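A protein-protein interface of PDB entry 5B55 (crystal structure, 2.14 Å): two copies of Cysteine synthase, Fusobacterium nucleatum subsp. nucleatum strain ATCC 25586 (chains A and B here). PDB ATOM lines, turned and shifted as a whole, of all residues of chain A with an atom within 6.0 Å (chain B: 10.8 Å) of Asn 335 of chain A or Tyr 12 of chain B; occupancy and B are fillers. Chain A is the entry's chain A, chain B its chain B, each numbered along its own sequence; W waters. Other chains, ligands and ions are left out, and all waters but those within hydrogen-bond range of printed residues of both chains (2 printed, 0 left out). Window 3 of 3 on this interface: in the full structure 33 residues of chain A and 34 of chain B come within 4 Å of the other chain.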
ATOM      1  N   MET A  22      -6.968 -21.964  18.341  1.00  0.00           N
ATOM      2  CA  MET A  22      -7.553 -21.365  17.200  1.00  0.00           C
ATOM      3  C   MET A  22      -6.825 -21.931  16.021  1.00  0.00           C
ATOM      4  O   MET A  22      -5.579 -21.848  15.924  1.00  0.00           O
ATOM      5  CB  MET A  22      -7.451 -19.854  17.241  1.00  0.00           C
ATOM      6  CG  MET A  22      -7.876 -19.148  15.946  1.00  0.00           C
ATOM      7  SD  MET A  22      -9.676 -19.061  15.791  1.00  0.00           S
ATOM      8  CE  MET A  22      -9.941 -17.439  16.516  1.00  0.00           C
ATOM      9  N   LEU A  23      -7.592 -22.475  15.096  1.00  0.00           N
ATOM     10  CA  LEU A  23      -7.031 -23.056  13.894  1.00  0.00           C
ATOM     11  C   LEU A  23      -7.302 -22.155  12.687  1.00  0.00           C
ATOM     12  O   LEU A  23      -8.421 -21.626  12.522  1.00  0.00           O
ATOM     13  CB  LEU A  23      -7.634 -24.422  13.634  1.00  0.00           C
ATOM     14  CG  LEU A  23      -7.697 -25.326  14.880  1.00  0.00           C
ATOM     15  CD1 LEU A  23      -8.945 -26.164  14.822  1.00  0.00           C
ATOM     16  CD2 LEU A  23      -6.515 -26.215  14.887  1.00  0.00           C
ATOM     17  N   GLU A  24      -6.334 -22.082  11.779  1.00  0.00           N
ATOM     18  CA  GLU A  24      -6.577 -21.532  10.441  1.00  0.00           C
ATOM     19  C   GLU A  24      -6.652 -22.689   9.485  1.00  0.00           C
ATOM     20  O   GLU A  24      -5.641 -23.412   9.247  1.00  0.00           O
ATOM     21  CB  GLU A  24      -5.475 -20.535  10.008  1.00  0.00           C
ATOM     22  CG  GLU A  24      -5.670 -20.055   8.554  1.00  0.00           C
ATOM     23  CD  GLU A  24      -4.580 -19.119   8.107  1.00  0.00           C
ATOM     24  OE1 GLU A  24      -3.576 -18.981   8.819  1.00  0.00           O
ATOM     25  OE2 GLU A  24      -4.695 -18.533   7.011  1.00  0.00           O
ATOM     26  N   LEU A  25      -7.833 -22.900   8.916  1.00  0.00           N
ATOM     27  CA  LEU A  25      -8.060 -24.012   8.030  1.00  0.00           C
ATOM     28  C   LEU A  25      -8.142 -23.550   6.586  1.00  0.00           C
ATOM     29  O   LEU A  25      -9.018 -22.765   6.254  1.00  0.00           O
ATOM     30  CB  LEU A  25      -9.375 -24.726   8.372  1.00  0.00           C
ATOM     31  CG  LEU A  25      -9.459 -25.221   9.806  1.00  0.00           C
ATOM     32  CD1 LEU A  25     -10.784 -25.944  10.013  1.00  0.00           C
ATOM     33  CD2 LEU A  25      -8.292 -26.157  10.163  1.00  0.00           C
ATOM     34  N   LEU A 176      -2.928 -11.653  14.802  1.00  0.00           N
ATOM     35  CA  LEU A 176      -2.639 -11.897  13.378  1.00  0.00           C
ATOM     36  C   LEU A 176      -2.847 -10.648  12.472  1.00  0.00           C
ATOM     37  O   LEU A 176      -2.738 -10.757  11.261  1.00  0.00           O
ATOM     38  CB  LEU A 176      -3.554 -13.009  12.850  1.00  0.00           C
ATOM     39  CG  LEU A 176      -3.415 -14.381  13.522  1.00  0.00           C
ATOM     40  CD1 LEU A 176      -4.564 -15.315  13.150  1.00  0.00           C
ATOM     41  CD2 LEU A 176      -2.096 -14.989  13.104  1.00  0.00           C
ATOM     42  N   GLU A 332      -5.137 -27.850   4.298  1.00  0.00           N
ATOM     43  CA  GLU A 332      -4.176 -27.924   5.421  1.00  0.00           C
ATOM     44  C   GLU A 332      -4.597 -27.096   6.596  1.00  0.00           C
ATOM     45  O   GLU A 332      -5.348 -26.083   6.463  1.00  0.00           O
ATOM     46  CB  GLU A 332      -2.738 -27.494   5.028  1.00  0.00           C
ATOM     47  CG  GLU A 332      -2.583 -26.055   4.578  1.00  0.00           C
ATOM     48  CD  GLU A 332      -1.137 -25.622   4.340  1.00  0.00           C
ATOM     49  OE1 GLU A 332      -0.241 -26.028   5.138  1.00  0.00           O
ATOM     50  OE2 GLU A 332      -0.914 -24.827   3.379  1.00  0.00           O
ATOM     51  N   ILE A 333      -4.086 -27.531   7.736  1.00  0.00           N
ATOM     52  CA  ILE A 333      -4.080 -26.700   8.931  1.00  0.00           C
ATOM     53  C   ILE A 333      -2.880 -25.801   8.737  1.00  0.00           C
ATOM     54  O   ILE A 333      -1.744 -26.245   8.831  1.00  0.00           O
ATOM     55  CB  ILE A 333      -4.024 -27.512  10.225  1.00  0.00           C
ATOM     56  CG1 ILE A 333      -5.189 -28.483  10.284  1.00  0.00           C
ATOM     57  CG2 ILE A 333      -3.998 -26.584  11.422  1.00  0.00           C
ATOM     58  CD1 ILE A 333      -5.250 -29.378  11.528  1.00  0.00           C
ATOM     59  N   MLY A 334      -3.172 -24.525   8.480  1.00  0.00           N
ATOM     60  CA  MLY A 334      -2.211 -23.523   8.097  1.00  0.00           C
ATOM     61  CB  MLY A 334      -2.884 -22.524   7.143  1.00  0.00           C
ATOM     62  CG  MLY A 334      -2.031 -21.384   6.585  1.00  0.00           C
ATOM     63  CD  MLY A 334      -0.799 -21.919   5.862  1.00  0.00           C
ATOM     64  CE  MLY A 334      -0.461 -21.089   4.634  1.00  0.00           C
ATOM     65  NZ  MLY A 334       0.086 -19.753   4.976  1.00  0.00           N
ATOM     66  C   MLY A 334      -1.607 -22.759   9.241  1.00  0.00           C
ATOM     67  O   MLY A 334      -0.500 -22.201   9.089  1.00  0.00           O
ATOM     68  N   ASN A 335      -2.298 -22.733  10.387  1.00  0.00           N
ATOM     69  CA  ASN A 335      -1.768 -22.150  11.619  1.00  0.00           C
ATOM     70  C   ASN A 335      -2.604 -22.672  12.820  1.00  0.00           C
ATOM     71  O   ASN A 335      -3.740 -23.070  12.637  1.00  0.00           O
ATOM     72  CB  ASN A 335      -1.873 -20.606  11.566  1.00  0.00           C
ATOM     73  CG  ASN A 335      -0.903 -19.891  12.531  1.00  0.00           C
ATOM     74  OD1 ASN A 335      -0.098 -20.545  13.220  1.00  0.00           O
ATOM     75  ND2 ASN A 335      -0.991 -18.530  12.600  1.00  0.00           N
ATOM     76  N   VAL A 336      -2.019 -22.661  14.009  1.00  0.00           N
ATOM     77  CA  VAL A 336      -2.693 -22.929  15.252  1.00  0.00           C
ATOM     78  C   VAL A 336      -2.097 -21.939  16.225  1.00  0.00           C
ATOM     79  O   VAL A 336      -0.873 -21.903  16.390  1.00  0.00           O
ATOM     80  CB  VAL A 336      -2.437 -24.365  15.723  1.00  0.00           C
ATOM     81  CG1 VAL A 336      -3.162 -24.646  17.034  1.00  0.00           C
ATOM     82  CG2 VAL A 336      -2.880 -25.356  14.661  1.00  0.00           C
ATOM     83  N   LEU A 337      -2.952 -21.140  16.841  1.00  0.00           N
ATOM     84  CA  LEU A 337      -2.608 -20.271  17.935  1.00  0.00           C
ATOM     85  C   LEU A 337      -3.166 -20.852  19.203  1.00  0.00           C
ATOM     86  O   LEU A 337      -4.284 -21.431  19.216  1.00  0.00           O
ATOM     87  CB  LEU A 337      -3.217 -18.862  17.790  1.00  0.00           C
ATOM     88  CG  LEU A 337      -3.024 -18.089  16.494  1.00  0.00           C
ATOM     89  CD1 LEU A 337      -3.663 -16.705  16.604  1.00  0.00           C
ATOM     90  CD2 LEU A 337      -1.555 -17.960  16.151  1.00  0.00           C
ATOM     91  N   GLN B   7       8.059 -27.947   9.365  1.00  0.00           N
ATOM     92  CA  GLN B   7       9.150 -27.283  10.178  1.00  0.00           C
ATOM     93  C   GLN B   7       8.701 -26.034  10.984  1.00  0.00           C
ATOM     94  O   GLN B   7       8.694 -26.017  12.232  1.00  0.00           O
ATOM     95  CB  GLN B   7      10.372 -26.973   9.301  1.00  0.00           C
ATOM     96  CG  GLN B   7      10.157 -27.030   7.777  1.00  0.00           C
ATOM     97  CD  GLN B   7      11.228 -26.316   6.944  1.00  0.00           C
ATOM     98  OE1 GLN B   7      11.645 -26.816   5.901  1.00  0.00           O
ATOM     99  NE2 GLN B   7      11.641 -25.136   7.379  1.00  0.00           N
ATOM    100  N   MLY B   8       8.357 -24.993  10.237  1.00  0.00           N
ATOM    101  CA  MLY B   8       7.499 -23.864  10.707  1.00  0.00           C
ATOM    102  CB  MLY B   8       7.263 -22.759   9.613  1.00  0.00           C
ATOM    103  CG  MLY B   8       7.689 -23.054   8.146  1.00  0.00           C
ATOM    104  CD  MLY B   8       6.889 -24.217   7.414  1.00  0.00           C
ATOM    105  CE  MLY B   8       6.900 -24.269   5.874  1.00  0.00           C
ATOM    106  NZ  MLY B   8       8.262 -24.444   5.314  1.00  0.00           N
ATOM    107  C   MLY B   8       6.138 -24.440  11.087  1.00  0.00           C
ATOM    108  O   MLY B   8       5.556 -24.084  12.091  1.00  0.00           O
ATOM    109  N   MLY B   9       5.673 -25.345  10.233  1.00  0.00           N
ATOM    110  CA  MLY B   9       4.482 -26.128  10.426  1.00  0.00           C
ATOM    111  CB  MLY B   9       4.307 -27.098   9.241  1.00  0.00           C
ATOM    112  CG  MLY B   9       3.135 -27.995   9.299  1.00  0.00           C
ATOM    113  CD  MLY B   9       3.040 -28.847   8.078  1.00  0.00           C
ATOM    114  CE  MLY B   9       1.911 -28.389   7.175  1.00  0.00           C
ATOM    115  NZ  MLY B   9       1.970 -29.119   5.851  1.00  0.00           N
ATOM    116  CH1 MLY B   9       1.414 -30.486   6.001  1.00  0.00           C
ATOM    117  CH2 MLY B   9       1.212 -28.378   4.834  1.00  0.00           C
ATOM    118  C   MLY B   9       4.557 -26.872  11.764  1.00  0.00           C
ATOM    119  O   MLY B   9       3.658 -26.762  12.564  1.00  0.00           O
ATOM    120  N   MET B  10       5.660 -27.570  12.017  1.00  0.00           N
ATOM    121  CA  MET B  10       5.799 -28.345  13.237  1.00  0.00           C
ATOM    122  C   MET B  10       5.791 -27.455  14.449  1.00  0.00           C
ATOM    123  O   MET B  10       5.232 -27.845  15.489  1.00  0.00           O
ATOM    124  CB  MET B  10       7.062 -29.212  13.236  1.00  0.00           C
ATOM    125  CG  MET B  10       7.085 -30.286  12.191  1.00  0.00           C
ATOM    126  SD  MET B  10       5.749 -31.503  12.227  1.00  0.00           S
ATOM    127  CE  MET B  10       6.328 -32.440  10.817  1.00  0.00           C
ATOM    128  N   MLY B  11       6.313 -26.238  14.311  1.00  0.00           N
ATOM    129  CA  MLY B  11       6.254 -25.309  15.408  1.00  0.00           C
ATOM    130  CB  MLY B  11       7.051 -24.016  15.167  1.00  0.00           C
ATOM    131  CG  MLY B  11       7.056 -23.047  16.369  1.00  0.00           C
ATOM    132  CD  MLY B  11       7.972 -23.459  17.516  1.00  0.00           C
ATOM    133  CE  MLY B  11       7.333 -23.283  18.883  1.00  0.00           C
ATOM    134  NZ  MLY B  11       6.220 -24.257  19.198  1.00  0.00           N
ATOM    135  C   MLY B  11       4.776 -25.008  15.763  1.00  0.00           C
ATOM    136  O   MLY B  11       4.434 -25.066  16.927  1.00  0.00           O
ATOM    137  N   TYR B  12       3.911 -24.680  14.804  1.00  0.00           N
ATOM    138  CA  TYR B  12       2.533 -24.299  15.218  1.00  0.00           C
ATOM    139  C   TYR B  12       1.671 -25.566  15.574  1.00  0.00           C
ATOM    140  O   TYR B  12       0.779 -25.503  16.414  1.00  0.00           O
ATOM    141  CB  TYR B  12       1.884 -23.329  14.213  1.00  0.00           C
ATOM    142  CG  TYR B  12       1.559 -23.886  12.815  1.00  0.00           C
ATOM    143  CD1 TYR B  12       0.553 -24.855  12.630  1.00  0.00           C
ATOM    144  CD2 TYR B  12       2.222 -23.387  11.667  1.00  0.00           C
ATOM    145  CE1 TYR B  12       0.233 -25.298  11.367  1.00  0.00           C
ATOM    146  CE2 TYR B  12       1.919 -23.843  10.406  1.00  0.00           C
ATOM    147  CZ  TYR B  12       0.927 -24.812  10.252  1.00  0.00           C
ATOM    148  OH  TYR B  12       0.646 -25.282   8.990  1.00  0.00           O
ATOM    149  N   LEU B  13       1.964 -26.708  14.960  1.00  0.00           N
ATOM    150  CA  LEU B  13       1.177 -27.908  15.214  1.00  0.00           C
ATOM    151  C   LEU B  13       1.348 -28.449  16.629  1.00  0.00           C
ATOM    152  O   LEU B  13       0.441 -29.090  17.162  1.00  0.00           O
ATOM    153  CB  LEU B  13       1.407 -28.994  14.194  1.00  0.00           C
ATOM    154  CG  LEU B  13       0.896 -28.758  12.817  1.00  0.00           C
ATOM    155  CD1 LEU B  13       1.305 -29.981  12.005  1.00  0.00           C
ATOM    156  CD2 LEU B  13      -0.614 -28.577  12.712  1.00  0.00           C
ATOM    157  N   GLU B  14       2.447 -28.104  17.276  1.00  0.00           N
ATOM    158  CA  GLU B  14       2.629 -28.401  18.678  1.00  0.00           C
ATOM    159  C   GLU B  14       1.606 -27.743  19.619  1.00  0.00           C
ATOM    160  O   GLU B  14       1.408 -28.223  20.724  1.00  0.00           O
ATOM    161  CB  GLU B  14       4.042 -28.030  19.088  1.00  0.00           C
ATOM    162  CG  GLU B  14       4.434 -28.531  20.471  1.00  0.00           C
ATOM    163  CD  GLU B  14       5.870 -28.182  20.884  1.00  0.00           C
ATOM    164  OE1 GLU B  14       6.483 -27.231  20.328  1.00  0.00           O
ATOM    165  OE2 GLU B  14       6.361 -28.867  21.811  1.00  0.00           O
ATOM    166  N   ASN B  15       0.974 -26.643  19.200  1.00  0.00           N
ATOM    167  CA  ASN B  15      -0.070 -26.017  19.973  1.00  0.00           C
ATOM    168  C   ASN B  15      -1.336 -26.894  20.098  1.00  0.00           C
ATOM    169  O   ASN B  15      -2.218 -26.542  20.798  1.00  0.00           O
ATOM    170  CB  ASN B  15      -0.440 -24.646  19.371  1.00  0.00           C
ATOM    171  CG  ASN B  15       0.680 -23.610  19.536  1.00  0.00           C
ATOM    172  OD1 ASN B  15       1.347 -23.549  20.543  1.00  0.00           O
ATOM    173  ND2 ASN B  15       0.875 -22.795  18.522  1.00  0.00           N
ATOM    174  N   LEU B  16      -1.420 -27.996  19.364  1.00  0.00           N
ATOM    175  CA  LEU B  16      -2.509 -28.959  19.464  1.00  0.00           C
ATOM    176  C   LEU B  16      -2.314 -30.030  20.550  1.00  0.00           C
ATOM    177  O   LEU B  16      -3.237 -30.826  20.783  1.00  0.00           O
ATOM    178  CB  LEU B  16      -2.683 -29.684  18.102  1.00  0.00           C
ATOM    179  CG  LEU B  16      -3.072 -28.783  16.942  1.00  0.00           C
ATOM    180  CD1 LEU B  16      -3.116 -29.557  15.615  1.00  0.00           C
ATOM    181  CD2 LEU B  16      -4.397 -28.057  17.156  1.00  0.00           C
ATOM    182  N   VAL B  17      -1.118 -30.105  21.132  1.00  0.00           N
ATOM    183  CA  VAL B  17      -0.816 -31.132  22.131  1.00  0.00           C
ATOM    184  C   VAL B  17      -0.203 -30.504  23.381  1.00  0.00           C
ATOM    185  O   VAL B  17       0.350 -29.403  23.309  1.00  0.00           O
ATOM    186  CB  VAL B  17       0.068 -32.252  21.616  1.00  0.00           C
ATOM    187  CG1 VAL B  17      -0.549 -32.835  20.379  1.00  0.00           C
ATOM    188  CG2 VAL B  17       1.509 -31.750  21.330  1.00  0.00           C
ATOM    189  N   GLY B  18      -0.346 -31.193  24.510  1.00  0.00           N
ATOM    190  CA  GLY B  18       0.301 -30.786  25.695  1.00  0.00           C
ATOM    191  C   GLY B  18      -0.303 -29.552  26.361  1.00  0.00           C
ATOM    192  O   GLY B  18      -1.448 -29.142  26.086  1.00  0.00           O
ATOM    193  N   MLY B  19       0.469 -29.046  27.322  1.00  0.00           N
ATOM    194  CA  MLY B  19       0.107 -27.918  28.160  1.00  0.00           C
ATOM    195  CB  MLY B  19       0.005 -26.598  27.329  1.00  0.00           C
ATOM    196  CG  MLY B  19       1.155 -26.323  26.342  1.00  0.00           C
ATOM    197  CD  MLY B  19       2.467 -26.120  27.038  1.00  0.00           C
ATOM    198  CE  MLY B  19       3.567 -25.437  26.135  1.00  0.00           C
ATOM    199  NZ  MLY B  19       5.000 -25.381  26.738  1.00  0.00           N
ATOM    200  CH1 MLY B  19       4.940 -24.948  28.158  1.00  0.00           C
ATOM    201  CH2 MLY B  19       5.840 -24.442  25.959  1.00  0.00           C
ATOM    202  C   MLY B  19      -1.194 -28.202  28.923  1.00  0.00           C
ATOM    203  O   MLY B  19      -2.090 -27.375  28.977  1.00  0.00           O
ATOM    204  N   LEU B  45      -5.318 -33.145  21.254  1.00  0.00           N
ATOM    205  CA  LEU B  45      -5.988 -33.347  19.898  1.00  0.00           C
ATOM    206  C   LEU B  45      -7.041 -34.414  19.773  1.00  0.00           C
ATOM    207  O   LEU B  45      -8.186 -34.138  19.379  1.00  0.00           O
ATOM    208  CB  LEU B  45      -4.950 -33.581  18.792  1.00  0.00           C
ATOM    209  CG  LEU B  45      -5.489 -33.596  17.350  1.00  0.00           C
ATOM    210  CD1 LEU B  45      -6.180 -32.300  16.993  1.00  0.00           C
ATOM    211  CD2 LEU B  45      -4.408 -33.929  16.378  1.00  0.00           C
ATOM    212  N   PHE B  55       2.893 -36.849  17.739  1.00  0.00           N
ATOM    213  CA  PHE B  55       3.390 -35.637  17.194  1.00  0.00           C
ATOM    214  C   PHE B  55       4.915 -35.642  17.287  1.00  0.00           C
ATOM    215  O   PHE B  55       5.570 -35.317  16.302  1.00  0.00           O
ATOM    216  CB  PHE B  55       2.837 -34.394  17.906  1.00  0.00           C
ATOM    217  CG  PHE B  55       3.481 -33.123  17.435  1.00  0.00           C
ATOM    218  CD1 PHE B  55       3.194 -32.614  16.191  1.00  0.00           C
ATOM    219  CD2 PHE B  55       4.418 -32.509  18.204  1.00  0.00           C
ATOM    220  CE1 PHE B  55       3.808 -31.453  15.723  1.00  0.00           C
ATOM    221  CE2 PHE B  55       5.056 -31.376  17.752  1.00  0.00           C
ATOM    222  CZ  PHE B  55       4.751 -30.852  16.508  1.00  0.00           C
ATOM    223  N   MLY B  59       7.460 -35.447  14.069  1.00  0.00           N
ATOM    224  CA  MLY B  59       8.338 -34.274  13.971  1.00  0.00           C
ATOM    225  CB  MLY B  59       8.124 -33.362  15.164  1.00  0.00           C
ATOM    226  CG  MLY B  59       9.086 -32.172  15.191  1.00  0.00           C
ATOM    227  CD  MLY B  59       8.645 -31.166  16.267  1.00  0.00           C
ATOM    228  CE  MLY B  59       9.822 -30.376  16.802  1.00  0.00           C
ATOM    229  NZ  MLY B  59       9.730 -28.898  17.143  1.00  0.00           N
ATOM    230  CH1 MLY B  59       8.340 -28.551  17.561  1.00  0.00           C
ATOM    231  CH2 MLY B  59      10.672 -28.572  18.219  1.00  0.00           C
ATOM    232  C   MLY B  59       9.862 -34.639  13.908  1.00  0.00           C
ATOM    233  O   MLY B  59      10.622 -34.095  13.115  1.00  0.00           O
ATOM    234  N   MET B  88      -2.834 -37.222  13.391  1.00  0.00           N
ATOM    235  CA  MET B  88      -1.653 -36.463  13.043  1.00  0.00           C
ATOM    236  C   MET B  88      -1.080 -36.831  11.663  1.00  0.00           C
ATOM    237  O   MET B  88      -0.612 -35.974  10.897  1.00  0.00           O
ATOM    238  CB  MET B  88      -0.608 -36.572  14.194  1.00  0.00           C
ATOM    239  CG  MET B  88       0.512 -35.541  14.160  1.00  0.00           C
ATOM    240  SD  MET B  88       0.063 -33.814  13.905  1.00  0.00           S
ATOM    241  CE  MET B  88      -0.421 -33.475  15.588  1.00  0.00           C
ATOM    242  N   ILE B  91      -3.308 -35.001   9.224  1.00  0.00           N
ATOM    243  CA  ILE B  91      -2.907 -33.599   9.174  1.00  0.00           C
ATOM    244  C   ILE B  91      -1.680 -33.394   8.279  1.00  0.00           C
ATOM    245  O   ILE B  91      -1.610 -32.418   7.537  1.00  0.00           O
ATOM    246  CB  ILE B  91      -2.632 -33.026  10.579  1.00  0.00           C
ATOM    247  CG1 ILE B  91      -3.954 -32.944  11.392  1.00  0.00           C
ATOM    248  CG2 ILE B  91      -1.965 -31.661  10.475  1.00  0.00           C
ATOM    249  CD1 ILE B  91      -3.725 -32.675  12.883  1.00  0.00           C
ATOM    250  N   LEU B  92      -0.728 -34.307   8.367  1.00  0.00           N
ATOM    251  CA  LEU B  92       0.534 -34.205   7.636  1.00  0.00           C
ATOM    252  C   LEU B  92       0.494 -34.860   6.241  1.00  0.00           C
ATOM    253  O   LEU B  92       1.510 -34.914   5.560  1.00  0.00           O
ATOM    254  CB  LEU B  92       1.665 -34.793   8.500  1.00  0.00           C
ATOM    255  CG  LEU B  92       1.904 -33.940   9.755  1.00  0.00           C
ATOM    256  CD1 LEU B  92       2.761 -34.670  10.748  1.00  0.00           C
ATOM    257  CD2 LEU B  92       2.551 -32.626   9.387  1.00  0.00           C
ATOM    258  N   GLY B  93      -0.656 -35.372   5.834  1.00  0.00           N
ATOM    259  CA  GLY B  93      -0.833 -35.886   4.466  1.00  0.00           C
ATOM    260  C   GLY B  93      -0.402 -37.331   4.281  1.00  0.00           C
ATOM    261  O   GLY B  93      -0.011 -37.694   3.174  1.00  0.00           O
HETATM  262  O   HOH W   1      -2.643 -30.030   7.375  1.00  0.00           O
HETATM  263  O   HOH W   2       1.699 -24.235   6.823  1.00  0.00           O
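OE1 of Glu 332 of chain A sits close to NZ of MLY 9 of chain B, 3.9 Å away. The backbone carbonyl oxygen of Ile 333 of chain A lies within hydrogen-bond range of the side-chain hydroxyl of Tyr 12 of chain B (2.6 Å). The side-chain amide nitrogen (ND2) of Asn 15 of chain B sits at hydrogen-bond distance from the backbone carbonyl oxygen (O) of Val 336 of chain A (2.9 Å). The side-chain hydroxyl (OH) of Tyr 12 of chain B sits close to O of MLY 334 of chain A (3.3 Å).
Among the printed residues, pairs that only touch across the chains: Leu 23 of chain A with Leu 16 of chain B, Ile 333 of chain A with Ile 91 of chain B, Asn 335 of chain A with Tyr 12 of chain B, Val 336 of chain A with Tyr 12 of chain B and Val 336 of chain A with Leu 16 of chain B.
Hydrophobic or aromatic side chains of chain A that line the printed part of chain B: Leu 23, Ile 333 and Val 336. Along chain A the printed residues that touch a printed residue of chain B span positions 23 to 336. Of the 20 printed residues of chain B, 5 touch a printed residue of chain A. Printed residues of chain B that touch a printed residue of chain A: MLY 9, Tyr 12, Asn 15, Leu 16 and Ile 91. Hydrophobic or aromatic side chains of chain B within 4 Å of the printed part of chain A: Tyr 12, Leu 16 and Ile 91.
No position is printed for both chains. Of the 9 pairs that touch across the chains among the printed residues, none has its exchanged pair printed and touching as well.
Water W1 bridges the backbone carbonyl oxygen of Ile 91 of chain B (2.6 Å) and the backbone NH of Ile 333 of chain A (2.9 Å). Water W2 bridges OH of Tyr 12 of chain B and OE1 of Glu 332 of chain A.
Of chain B, only Tyr 12 (3.6 Å) comes within 4 Å of Asn 335 of chain A. No residue of chain B comes within 4 Å of Glu 24 of chain A. Ile 333 of chain A touches two residues of chain B. Of chain B, only Tyr 12 (3.2 Å) comes within 4 Å of MLY 334 of chain A. Val 336 of chain A touches just these residues of chain B: Tyr 12, Asn 15 and Leu 16. Leu 337 of chain A touches none of the printed residues of chain B. Of the printed residues of chain A, MLY 9 of chain B touches Glu 332. Printed residues of chain B within 4 Å of Glu 332 of chain A: MLY 9 (2.8 Å). Printed residues of chain A within 4 Å of Asn 15 of chain B: Val 336 (2.9 Å). Leu 176 of chain A touches none of the printed residues of chain B.
The backbone NH of Glu 24 of chain A lies within hydrogen-bond range of the backbone carbonyl oxygen of Asn 335 of chain A, 2.9 Å away. O of Tyr 12 of chain B sits close to ND2 of Asn 15 of chain B. O of Leu 16 of chain B lies within hydrogen-bond range of N of Leu 45 of chain B, at 3.2 Å. N of MLY 334 of chain A is in hydrogen-bond range of the backbone carbonyl oxygen of Glu 24 of chain A, 2.8 Å away.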
